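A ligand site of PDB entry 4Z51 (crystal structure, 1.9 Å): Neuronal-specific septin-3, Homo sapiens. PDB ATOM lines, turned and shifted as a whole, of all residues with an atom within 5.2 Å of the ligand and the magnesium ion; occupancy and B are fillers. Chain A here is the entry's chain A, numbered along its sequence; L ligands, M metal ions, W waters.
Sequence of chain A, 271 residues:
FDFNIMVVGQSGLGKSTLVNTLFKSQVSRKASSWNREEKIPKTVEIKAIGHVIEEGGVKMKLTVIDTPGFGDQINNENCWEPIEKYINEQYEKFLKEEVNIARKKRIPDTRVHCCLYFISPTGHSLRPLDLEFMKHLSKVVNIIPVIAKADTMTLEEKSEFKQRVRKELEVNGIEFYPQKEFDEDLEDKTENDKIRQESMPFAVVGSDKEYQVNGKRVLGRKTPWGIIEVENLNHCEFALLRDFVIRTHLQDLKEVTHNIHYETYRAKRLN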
ATOM      1  N   GLY A   9      13.163 -19.540 -22.003  1.00  0.00           N
ATOM      2  CA  GLY A   9      12.136 -18.784 -21.335  1.00  0.00           C
ATOM      3  C   GLY A   9      11.210 -19.680 -20.540  1.00  0.00           C
ATOM      4  O   GLY A   9      11.252 -20.908 -20.673  1.00  0.00           O
ATOM      5  N   GLN A  10      10.367 -19.059 -19.726  1.00  0.00           N
ATOM      6  CA  GLN A  10       9.396 -19.805 -18.926  1.00  0.00           C
ATOM      7  C   GLN A  10       8.519 -20.738 -19.777  1.00  0.00           C
ATOM      8  O   GLN A  10       8.196 -20.444 -20.932  1.00  0.00           O
ATOM      9  CB  GLN A  10       8.520 -18.827 -18.137  1.00  0.00           C
ATOM     10  CG  GLN A  10       7.530 -19.497 -17.223  1.00  0.00           C
ATOM     11  CD  GLN A  10       7.143 -18.617 -16.057  1.00  0.00           C
ATOM     12  OE1 GLN A  10       7.516 -18.883 -14.904  1.00  0.00           O
ATOM     13  NE2 GLN A  10       6.404 -17.549 -16.337  1.00  0.00           N
ATOM     14  N   SER A  11       8.154 -21.881 -19.198  1.00  0.00           N
ATOM     15  CA  SER A  11       7.282 -22.833 -19.872  1.00  0.00           C
ATOM     16  C   SER A  11       5.956 -22.180 -20.276  1.00  0.00           C
ATOM     17  O   SER A  11       5.387 -21.396 -19.517  1.00  0.00           O
ATOM     18  CB  SER A  11       7.013 -24.039 -18.965  1.00  0.00           C
ATOM     19  OG  SER A  11       6.087 -24.915 -19.578  1.00  0.00           O
ATOM     20  N   GLY A  12       5.469 -22.524 -21.460  1.00  0.00           N
ATOM     21  CA  GLY A  12       4.159 -22.082 -21.911  1.00  0.00           C
ATOM     22  C   GLY A  12       4.118 -20.720 -22.599  1.00  0.00           C
ATOM     23  O   GLY A  12       3.041 -20.172 -22.814  1.00  0.00           O
ATOM     24  N   LEU A  13       5.286 -20.190 -22.946  1.00  0.00           N
ATOM     25  CA  LEU A  13       5.341 -18.865 -23.564  1.00  0.00           C
ATOM     26  C   LEU A  13       5.293 -18.896 -25.102  1.00  0.00           C
ATOM     27  O   LEU A  13       5.298 -17.847 -25.756  1.00  0.00           O
ATOM     28  CB  LEU A  13       6.617 -18.125 -23.114  1.00  0.00           C
ATOM     29  CG  LEU A  13       6.626 -17.670 -21.649  1.00  0.00           C
ATOM     30  CD1 LEU A  13       7.889 -16.865 -21.335  1.00  0.00           C
ATOM     31  CD2 LEU A  13       5.373 -16.880 -21.297  1.00  0.00           C
ATOM     32  N   GLY A  14       5.258 -20.093 -25.673  1.00  0.00           N
ATOM     33  CA  GLY A  14       5.160 -20.238 -27.125  1.00  0.00           C
ATOM     34  C   GLY A  14       6.492 -20.387 -27.835  1.00  0.00           C
ATOM     35  O   GLY A  14       6.600 -20.114 -29.033  1.00  0.00           O
ATOM     36  N   LYS A  15       7.518 -20.826 -27.101  1.00  0.00           N
ATOM     37  CA  LYS A  15       8.856 -20.987 -27.673  1.00  0.00           C
ATOM     38  C   LYS A  15       8.883 -21.982 -28.829  1.00  0.00           C
ATOM     39  O   LYS A  15       9.365 -21.653 -29.912  1.00  0.00           O
ATOM     40  CB  LYS A  15       9.840 -21.422 -26.568  1.00  0.00           C
ATOM     41  CG  LYS A  15      10.045 -20.363 -25.477  1.00  0.00           C
ATOM     42  CD  LYS A  15      11.134 -20.768 -24.483  1.00  0.00           C
ATOM     43  CE  LYS A  15      10.868 -22.131 -23.847  1.00  0.00           C
ATOM     44  NZ  LYS A  15       9.593 -22.170 -23.086  1.00  0.00           N
ATOM     45  N   SER A  16       8.370 -23.188 -28.603  1.00  0.00           N
ATOM     46  CA  SER A  16       8.340 -24.216 -29.632  1.00  0.00           C
ATOM     47  C   SER A  16       7.480 -23.802 -30.832  1.00  0.00           C
ATOM     48  O   SER A  16       7.809 -24.119 -31.971  1.00  0.00           O
ATOM     49  CB  SER A  16       7.819 -25.538 -29.058  1.00  0.00           C
ATOM     50  OG  SER A  16       8.682 -26.029 -28.041  1.00  0.00           O
ATOM     51  N   THR A  17       6.391 -23.090 -30.565  1.00  0.00           N
ATOM     52  CA  THR A  17       5.528 -22.601 -31.623  1.00  0.00           C
ATOM     53  C   THR A  17       6.307 -21.596 -32.483  1.00  0.00           C
ATOM     54  O   THR A  17       6.198 -21.608 -33.708  1.00  0.00           O
ATOM     55  CB  THR A  17       4.226 -21.960 -31.067  1.00  0.00           C
ATOM     56  OG1 THR A  17       3.510 -22.923 -30.279  1.00  0.00           O
ATOM     57  CG2 THR A  17       3.319 -21.482 -32.202  1.00  0.00           C
ATOM     58  N   LEU A  18       7.099 -20.732 -31.850  1.00  0.00           N
ATOM     59  CA  LEU A  18       7.875 -19.735 -32.603  1.00  0.00           C
ATOM     60  C   LEU A  18       8.983 -20.400 -33.419  1.00  0.00           C
ATOM     61  O   LEU A  18       9.314 -19.931 -34.497  1.00  0.00           O
ATOM     62  CB  LEU A  18       8.480 -18.677 -31.670  1.00  0.00           C
ATOM     63  CG  LEU A  18       8.821 -17.391 -32.453  1.00  0.00           C
ATOM     64  CD1 LEU A  18       7.541 -16.657 -32.832  1.00  0.00           C
ATOM     65  CD2 LEU A  18       9.748 -16.483 -31.679  1.00  0.00           C
ATOM     66  N   ILE A  40       1.682 -29.120 -31.050  1.00  0.00           N
ATOM     67  CA  ILE A  40       3.073 -29.117 -30.625  1.00  0.00           C
ATOM     68  C   ILE A  40       3.165 -29.561 -29.159  1.00  0.00           C
ATOM     69  O   ILE A  40       2.542 -28.969 -28.291  1.00  0.00           O
ATOM     70  CB  ILE A  40       3.714 -27.730 -30.809  1.00  0.00           C
ATOM     71  CG1 ILE A  40       3.712 -27.349 -32.291  1.00  0.00           C
ATOM     72  CG2 ILE A  40       5.121 -27.695 -30.221  1.00  0.00           C
ATOM     73  CD1 ILE A  40       4.176 -25.918 -32.572  1.00  0.00           C
ATOM     74  N   PRO A  41       3.943 -30.628 -28.896  1.00  0.00           N
ATOM     75  CA  PRO A  41       4.018 -31.174 -27.542  1.00  0.00           C
ATOM     76  C   PRO A  41       4.836 -30.307 -26.591  1.00  0.00           C
ATOM     77  O   PRO A  41       5.713 -29.570 -27.049  1.00  0.00           O
ATOM     78  CB  PRO A  41       4.706 -32.527 -27.759  1.00  0.00           C
ATOM     79  CG  PRO A  41       5.573 -32.302 -28.951  1.00  0.00           C
ATOM     80  CD  PRO A  41       4.808 -31.352 -29.840  1.00  0.00           C
ATOM     81  N   LYS A  42       4.547 -30.385 -25.301  1.00  0.00           N
ATOM     82  CA  LYS A  42       5.380 -29.715 -24.310  1.00  0.00           C
ATOM     83  C   LYS A  42       6.807 -30.250 -24.423  1.00  0.00           C
ATOM     84  O   LYS A  42       7.010 -31.444 -24.617  1.00  0.00           O
ATOM     85  CB  LYS A  42       4.827 -29.933 -22.895  1.00  0.00           C
ATOM     86  CG  LYS A  42       5.473 -29.088 -21.815  1.00  0.00           C
ATOM     87  CD  LYS A  42       6.455 -29.891 -20.984  1.00  0.00           C
ATOM     88  CE  LYS A  42       7.201 -29.020 -19.987  1.00  0.00           C
ATOM     89  NZ  LYS A  42       8.153 -28.066 -20.644  1.00  0.00           N
ATOM     90  N   THR A  43       7.785 -29.360 -24.331  1.00  0.00           N
ATOM     91  CA  THR A  43       9.175 -29.748 -24.569  1.00  0.00           C
ATOM     92  C   THR A  43       9.818 -30.300 -23.307  1.00  0.00           C
ATOM     93  O   THR A  43       9.871 -29.625 -22.284  1.00  0.00           O
ATOM     94  CB  THR A  43       9.988 -28.539 -25.088  1.00  0.00           C
ATOM     95  OG1 THR A  43       9.268 -27.913 -26.149  1.00  0.00           O
ATOM     96  CG2 THR A  43      11.353 -28.985 -25.598  1.00  0.00           C
ATOM     97  N   ASP A  66      15.609 -25.892 -29.318  1.00  0.00           N
ATOM     98  CA  ASP A  66      14.433 -25.762 -28.471  1.00  0.00           C
ATOM     99  C   ASP A  66      14.803 -26.268 -27.079  1.00  0.00           C
ATOM    100  O   ASP A  66      15.551 -27.233 -26.938  1.00  0.00           O
ATOM    101  CB  ASP A  66      13.265 -26.565 -29.047  1.00  0.00           C
ATOM    102  CG  ASP A  66      11.905 -26.058 -28.569  1.00  0.00           C
ATOM    103  OD1 ASP A  66      11.859 -25.104 -27.766  1.00  0.00           O
ATOM    104  OD2 ASP A  66      10.869 -26.643 -28.997  1.00  0.00           O
ATOM    105  N   THR A  67      14.289 -25.601 -26.050  1.00  0.00           N
ATOM    106  CA  THR A  67      14.626 -25.931 -24.679  1.00  0.00           C
ATOM    107  C   THR A  67      13.365 -26.065 -23.835  1.00  0.00           C
ATOM    108  O   THR A  67      12.388 -25.339 -24.055  1.00  0.00           O
ATOM    109  CB  THR A  67      15.545 -24.870 -24.037  1.00  0.00           C
ATOM    110  OG1 THR A  67      14.861 -23.612 -24.012  1.00  0.00           O
ATOM    111  CG2 THR A  67      16.871 -24.738 -24.799  1.00  0.00           C
ATOM    112  N   PRO A  68      13.364 -26.999 -22.866  1.00  0.00           N
ATOM    113  CA  PRO A  68      12.257 -27.062 -21.912  1.00  0.00           C
ATOM    114  C   PRO A  68      12.152 -25.755 -21.156  1.00  0.00           C
ATOM    115  O   PRO A  68      13.184 -25.240 -20.700  1.00  0.00           O
ATOM    116  CB  PRO A  68      12.642 -28.212 -20.980  1.00  0.00           C
ATOM    117  CG  PRO A  68      13.668 -28.997 -21.726  1.00  0.00           C
ATOM    118  CD  PRO A  68      14.409 -28.001 -22.574  1.00  0.00           C
ATOM    119  N   GLY A  69      10.958 -25.209 -21.023  1.00  0.00           N
ATOM    120  CA  GLY A  69      10.777 -23.981 -20.280  1.00  0.00           C
ATOM    121  C   GLY A  69      11.103 -24.184 -18.807  1.00  0.00           C
ATOM    122  O   GLY A  69      11.058 -25.308 -18.301  1.00  0.00           O
ATOM    123  N   LYS A 149       3.862 -13.937 -26.830  1.00  0.00           N
ATOM    124  CA  LYS A 149       2.403 -13.854 -26.894  1.00  0.00           C
ATOM    125  C   LYS A 149       1.925 -12.423 -26.867  1.00  0.00           C
ATOM    126  O   LYS A 149       1.087 -12.067 -26.033  1.00  0.00           O
ATOM    127  CB  LYS A 149       1.766 -14.647 -25.735  1.00  0.00           C
ATOM    128  CG  LYS A 149       2.080 -16.143 -25.727  1.00  0.00           C
ATOM    129  CD  LYS A 149       1.278 -16.875 -24.652  1.00  0.00           C
ATOM    130  CE  LYS A 149       1.360 -18.384 -24.841  1.00  0.00           C
ATOM    131  NZ  LYS A 149       0.581 -19.157 -23.815  1.00  0.00           N
ATOM    132  N   ALA A 150       2.472 -11.594 -27.751  1.00  0.00           N
ATOM    133  CA  ALA A 150       2.203 -10.158 -27.766  1.00  0.00           C
ATOM    134  C   ALA A 150       0.734  -9.841 -28.035  1.00  0.00           C
ATOM    135  O   ALA A 150       0.273  -8.744 -27.757  1.00  0.00           O
ATOM    136  CB  ALA A 150       3.078  -9.459 -28.805  1.00  0.00           C
ATOM    137  N   ASP A 151       0.013 -10.810 -28.580  1.00  0.00           N
ATOM    138  CA  ASP A 151      -1.410 -10.635 -28.825  1.00  0.00           C
ATOM    139  C   ASP A 151      -2.190 -10.485 -27.517  1.00  0.00           C
ATOM    140  O   ASP A 151      -3.340 -10.039 -27.515  1.00  0.00           O
ATOM    141  CB  ASP A 151      -1.951 -11.823 -29.620  1.00  0.00           C
ATOM    142  CG  ASP A 151      -1.687 -13.138 -28.943  1.00  0.00           C
ATOM    143  OD1 ASP A 151      -0.500 -13.479 -28.742  1.00  0.00           O
ATOM    144  OD2 ASP A 151      -2.665 -13.847 -28.607  1.00  0.00           O
ATOM    145  N   THR A 152      -1.575 -10.848 -26.396  1.00  0.00           N
ATOM    146  CA  THR A 152      -2.284 -10.717 -25.127  1.00  0.00           C
ATOM    147  C   THR A 152      -2.257  -9.263 -24.603  1.00  0.00           C
ATOM    148  O   THR A 152      -2.889  -8.954 -23.591  1.00  0.00           O
ATOM    149  CB  THR A 152      -1.709 -11.712 -24.092  1.00  0.00           C
ATOM    150  OG1 THR A 152      -0.460 -11.242 -23.598  1.00  0.00           O
ATOM    151  CG2 THR A 152      -1.464 -13.047 -24.743  1.00  0.00           C
ATOM    152  N   VAL A 204       6.332 -10.481 -30.126  1.00  0.00           N
ATOM    153  CA  VAL A 204       6.032 -11.448 -31.170  1.00  0.00           C
ATOM    154  C   VAL A 204       4.781 -12.296 -30.917  1.00  0.00           C
ATOM    155  O   VAL A 204       4.325 -12.456 -29.785  1.00  0.00           O
ATOM    156  CB  VAL A 204       7.227 -12.411 -31.386  1.00  0.00           C
ATOM    157  CG1 VAL A 204       8.519 -11.609 -31.582  1.00  0.00           C
ATOM    158  CG2 VAL A 204       7.352 -13.393 -30.227  1.00  0.00           C
ATOM    159  N   VAL A 205       4.223 -12.799 -32.018  1.00  0.00           N
ATOM    160  CA  VAL A 205       3.163 -13.797 -31.994  1.00  0.00           C
ATOM    161  C   VAL A 205       3.653 -14.976 -32.829  1.00  0.00           C
ATOM    162  O   VAL A 205       4.267 -14.773 -33.882  1.00  0.00           O
ATOM    163  CB  VAL A 205       1.830 -13.241 -32.568  1.00  0.00           C
ATOM    164  CG1 VAL A 205       0.763 -14.340 -32.636  1.00  0.00           C
ATOM    165  CG2 VAL A 205       1.354 -12.071 -31.735  1.00  0.00           C
ATOM    166  N   GLY A 206       3.419 -16.185 -32.342  1.00  0.00           N
ATOM    167  CA  GLY A 206       3.825 -17.373 -33.060  1.00  0.00           C
ATOM    168  C   GLY A 206       2.617 -18.185 -33.487  1.00  0.00           C
ATOM    169  O   GLY A 206       1.585 -18.193 -32.813  1.00  0.00           O
ATOM    170  N   ARG A 221      -3.276 -16.768 -35.874  1.00  0.00           N
ATOM    171  CA  ARG A 221      -4.115 -17.373 -34.838  1.00  0.00           C
ATOM    172  C   ARG A 221      -5.548 -16.892 -35.025  1.00  0.00           C
ATOM    173  O   ARG A 221      -5.794 -15.690 -35.171  1.00  0.00           O
ATOM    174  CB  ARG A 221      -3.594 -17.012 -33.431  1.00  0.00           C
ATOM    175  CG  ARG A 221      -2.222 -17.596 -33.089  1.00  0.00           C
ATOM    176  CD  ARG A 221      -1.711 -17.157 -31.709  1.00  0.00           C
ATOM    177  NE  ARG A 221      -2.710 -17.353 -30.668  1.00  0.00           N
ATOM    178  CZ  ARG A 221      -2.970 -18.517 -30.075  1.00  0.00           C
ATOM    179  NH1 ARG A 221      -2.295 -19.612 -30.388  1.00  0.00           N
ATOM    180  NH2 ARG A 221      -3.916 -18.577 -29.141  1.00  0.00           N
HETATM  181  P1  LIG L   1       7.500 -25.410 -23.006  1.00  0.00           P
HETATM  182  O1  LIG L   1       8.667 -24.527 -22.638  1.00  0.00           O
HETATM  183  O2  LIG L   1       7.830 -26.493 -23.995  1.00  0.00           O
HETATM  184  O3  LIG L   1       6.835 -26.112 -21.853  1.00  0.00           O
HETATM  185  N1  LIG L   1       6.376 -24.472 -23.680  1.00  0.00           N
HETATM  186  P2  LIG L   1       6.568 -23.521 -24.969  1.00  0.00           P
HETATM  187  O4  LIG L   1       7.287 -24.271 -26.022  1.00  0.00           O
HETATM  188  O5  LIG L   1       7.178 -22.239 -24.580  1.00  0.00           O
HETATM  189  O6  LIG L   1       5.156 -23.162 -25.496  1.00  0.00           O
HETATM  190  P3  LIG L   1       4.381 -23.764 -26.706  1.00  0.00           P
HETATM  191  O7  LIG L   1       4.969 -23.337 -27.994  1.00  0.00           O
HETATM  192  O8  LIG L   1       4.151 -25.206 -26.496  1.00  0.00           O
HETATM  193  O9  LIG L   1       2.969 -23.070 -26.687  1.00  0.00           O
HETATM  194  C1  LIG L   1       2.133 -23.126 -25.516  1.00  0.00           C
HETATM  195  C2  LIG L   1       0.704 -22.705 -25.853  1.00  0.00           C
HETATM  196  O10 LIG L   1       0.669 -21.313 -26.237  1.00  0.00           O
HETATM  197  C3  LIG L   1       0.056 -23.470 -27.005  1.00  0.00           C
HETATM  198  O11 LIG L   1      -1.325 -23.629 -26.723  1.00  0.00           O
HETATM  199  C4  LIG L   1       0.279 -22.523 -28.187  1.00  0.00           C
HETATM  200  O12 LIG L   1      -0.631 -22.698 -29.245  1.00  0.00           O
HETATM  201  C5  LIG L   1       0.051 -21.180 -27.506  1.00  0.00           C
HETATM  202  N2  LIG L   1       0.728 -20.080 -28.191  1.00  0.00           N
HETATM  203  C6  LIG L   1       1.913 -20.164 -28.877  1.00  0.00           C
HETATM  204  N3  LIG L   1       2.294 -19.010 -29.384  1.00  0.00           N
HETATM  205  C7  LIG L   1       1.306 -18.128 -28.990  1.00  0.00           C
HETATM  206  C8  LIG L   1       1.181 -16.740 -29.222  1.00  0.00           C
HETATM  207  O13 LIG L   1       1.951 -16.006 -29.852  1.00  0.00           O
HETATM  208  N4  LIG L   1       0.032 -16.213 -28.634  1.00  0.00           N
HETATM  209  C9  LIG L   1      -0.883 -16.929 -27.907  1.00  0.00           C
HETATM  210  N5  LIG L   1      -1.942 -16.239 -27.430  1.00  0.00           N
HETATM  211  N6  LIG L   1      -0.780 -18.230 -27.675  1.00  0.00           N
HETATM  212  C10 LIG L   1       0.329 -18.758 -28.245  1.00  0.00           C
HETATM  213 MG    MG M   1       8.228 -26.071 -25.943  1.00  0.00          MG
HETATM  214  O   HOH W   1      -2.859 -21.794 -25.249  1.00  0.00           O
HETATM  215  O   HOH W   2       6.364 -26.983 -26.602  1.00  0.00           O
HETATM  216  O   HOH W   3      10.081 -25.118 -25.689  1.00  0.00           O
HETATM  217  O   HOH W   4       1.969 -26.650 -27.381  1.00  0.00           O
HETATM  218  O   HOH W   5       1.146 -23.818 -31.245  1.00  0.00           O
HETATM  219  O   HOH W   6       4.983 -18.059 -30.001  1.00  0.00           O
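N of Thr 43 lies close to O2 of the ligand, at 2.9 Å.
The backbone NH (N) of Ser 16 is in hydrogen-bond range of an oxygen (O7) of the ligand (3.5 Å).
An oxygen (O5) of the ligand lies within hydrogen-bond range of the backbone NH of Lys 15.
An oxygen (O1) of the ligand is in salt-bridge range of the side-chain amino group (NZ) of Lys 15 (2.6 Å).
The side-chain amino group of Lys 42 lies within salt-bridge range of an oxygen (O3) of the ligand.
OG of Ser 11 lies within hydrogen-bond range of O3 of the ligand, at 2.7 Å.
O7 of the ligand sits at hydrogen-bond distance from N of Thr 17 (2.9 Å).
The side-chain hydroxyl of Thr 17 lies within hydrogen-bond range of an oxygen (O7) of the ligand.
OD2 of Asp 151 lies within hydrogen-bond range of N5 of the ligand, 2.8 Å away.
An oxygen (O1) of the ligand lies within hydrogen-bond range of the backbone NH of Gly 69 (2.9 Å).
N of Gly 206 lies within hydrogen-bond range of O13 of the ligand, at 2.9 Å.
An oxygen (O6) of the ligand lies within hydrogen-bond range of the backbone NH of Gly 14.
The backbone NH (N) of Leu 13 is in hydrogen-bond range of an oxygen (O5) of the ligand, 3.2 Å away.
O10 of the ligand sits at hydrogen-bond distance from NZ of Lys 149 (3.2 Å).
The guanidinium group of Arg 221 sits close to a nitrogen (N6) of the ligand.
The side-chain hydroxyl (OG) of Ser 16 lies close to the side-chain carboxylate (OD2) of Asp 66.
O of Gln 10 sits at hydrogen-bond distance from NZ of Lys 15, at 3.1 Å.
The side-chain amino group of Lys 15 sits at hydrogen-bond distance from the backbone carbonyl oxygen of Gly 9.
NZ of Lys 149 lies within hydrogen-bond range of O of Gly 12 (2.8 Å).
The backbone carbonyl oxygen of Lys 149 sits at hydrogen-bond distance from the side-chain hydroxyl of Thr 152 (3.0 Å).
The backbone carbonyl oxygen (O) of Val 204 sits at hydrogen-bond distance from the backbone NH (N) of Lys 149.
The backbone NH of Gly 12 lies close to a nitrogen (N1) of the ligand (3.1 Å).
Merely in contact with the ligand: Val 205 and Pro 68.
16 residues have an atom within 4 Å of the ligand: Ser 11, Gly 12, Leu 13, Gly 14, Lys 15, Ser 16, Thr 17, Lys 42, Thr 43, Pro 68, Gly 69, Lys 149, Asp 151, Val 205, Gly 206 and Arg 221.
Of the 26 residues printed, 2 come within 4 Å of the magnesium ion.
The nearest printed residue that does not touch the magnesium ion is Asp 66 (4.1 Å).
The magnesium ion is bound by an oxygen (O2) of the ligand (2.0 Å), an oxygen (O4) of the ligand (2.0 Å), water W3 (2.1 Å), the side-chain hydroxyl (OG1) of Thr 43 (2.1 Å), the side-chain hydroxyl (OG) of Ser 16 (2.1 Å) and water W2 (2.2 Å).
The magnesium ion has six donor atoms within binding distance.
Water W3 lies within hydrogen-bond range of OD1 of Asp 66, O of Thr 67 and O1 of the ligand.
Water W2 lies within hydrogen-bond range of the backbone carbonyl oxygen of Pro 41 and an oxygen (O8) of the ligand.
Water W4 bridges O of Ile 40 (2.6 Å) and O8 of the ligand (2.8 Å).
Water W5 bridges OG1 of Thr 17 (2.7 Å) and O12 of the ligand (2.9 Å).
Water W6 lies within hydrogen-bond range of O of Gly 14, N3 of the ligand and N of Gly 206.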
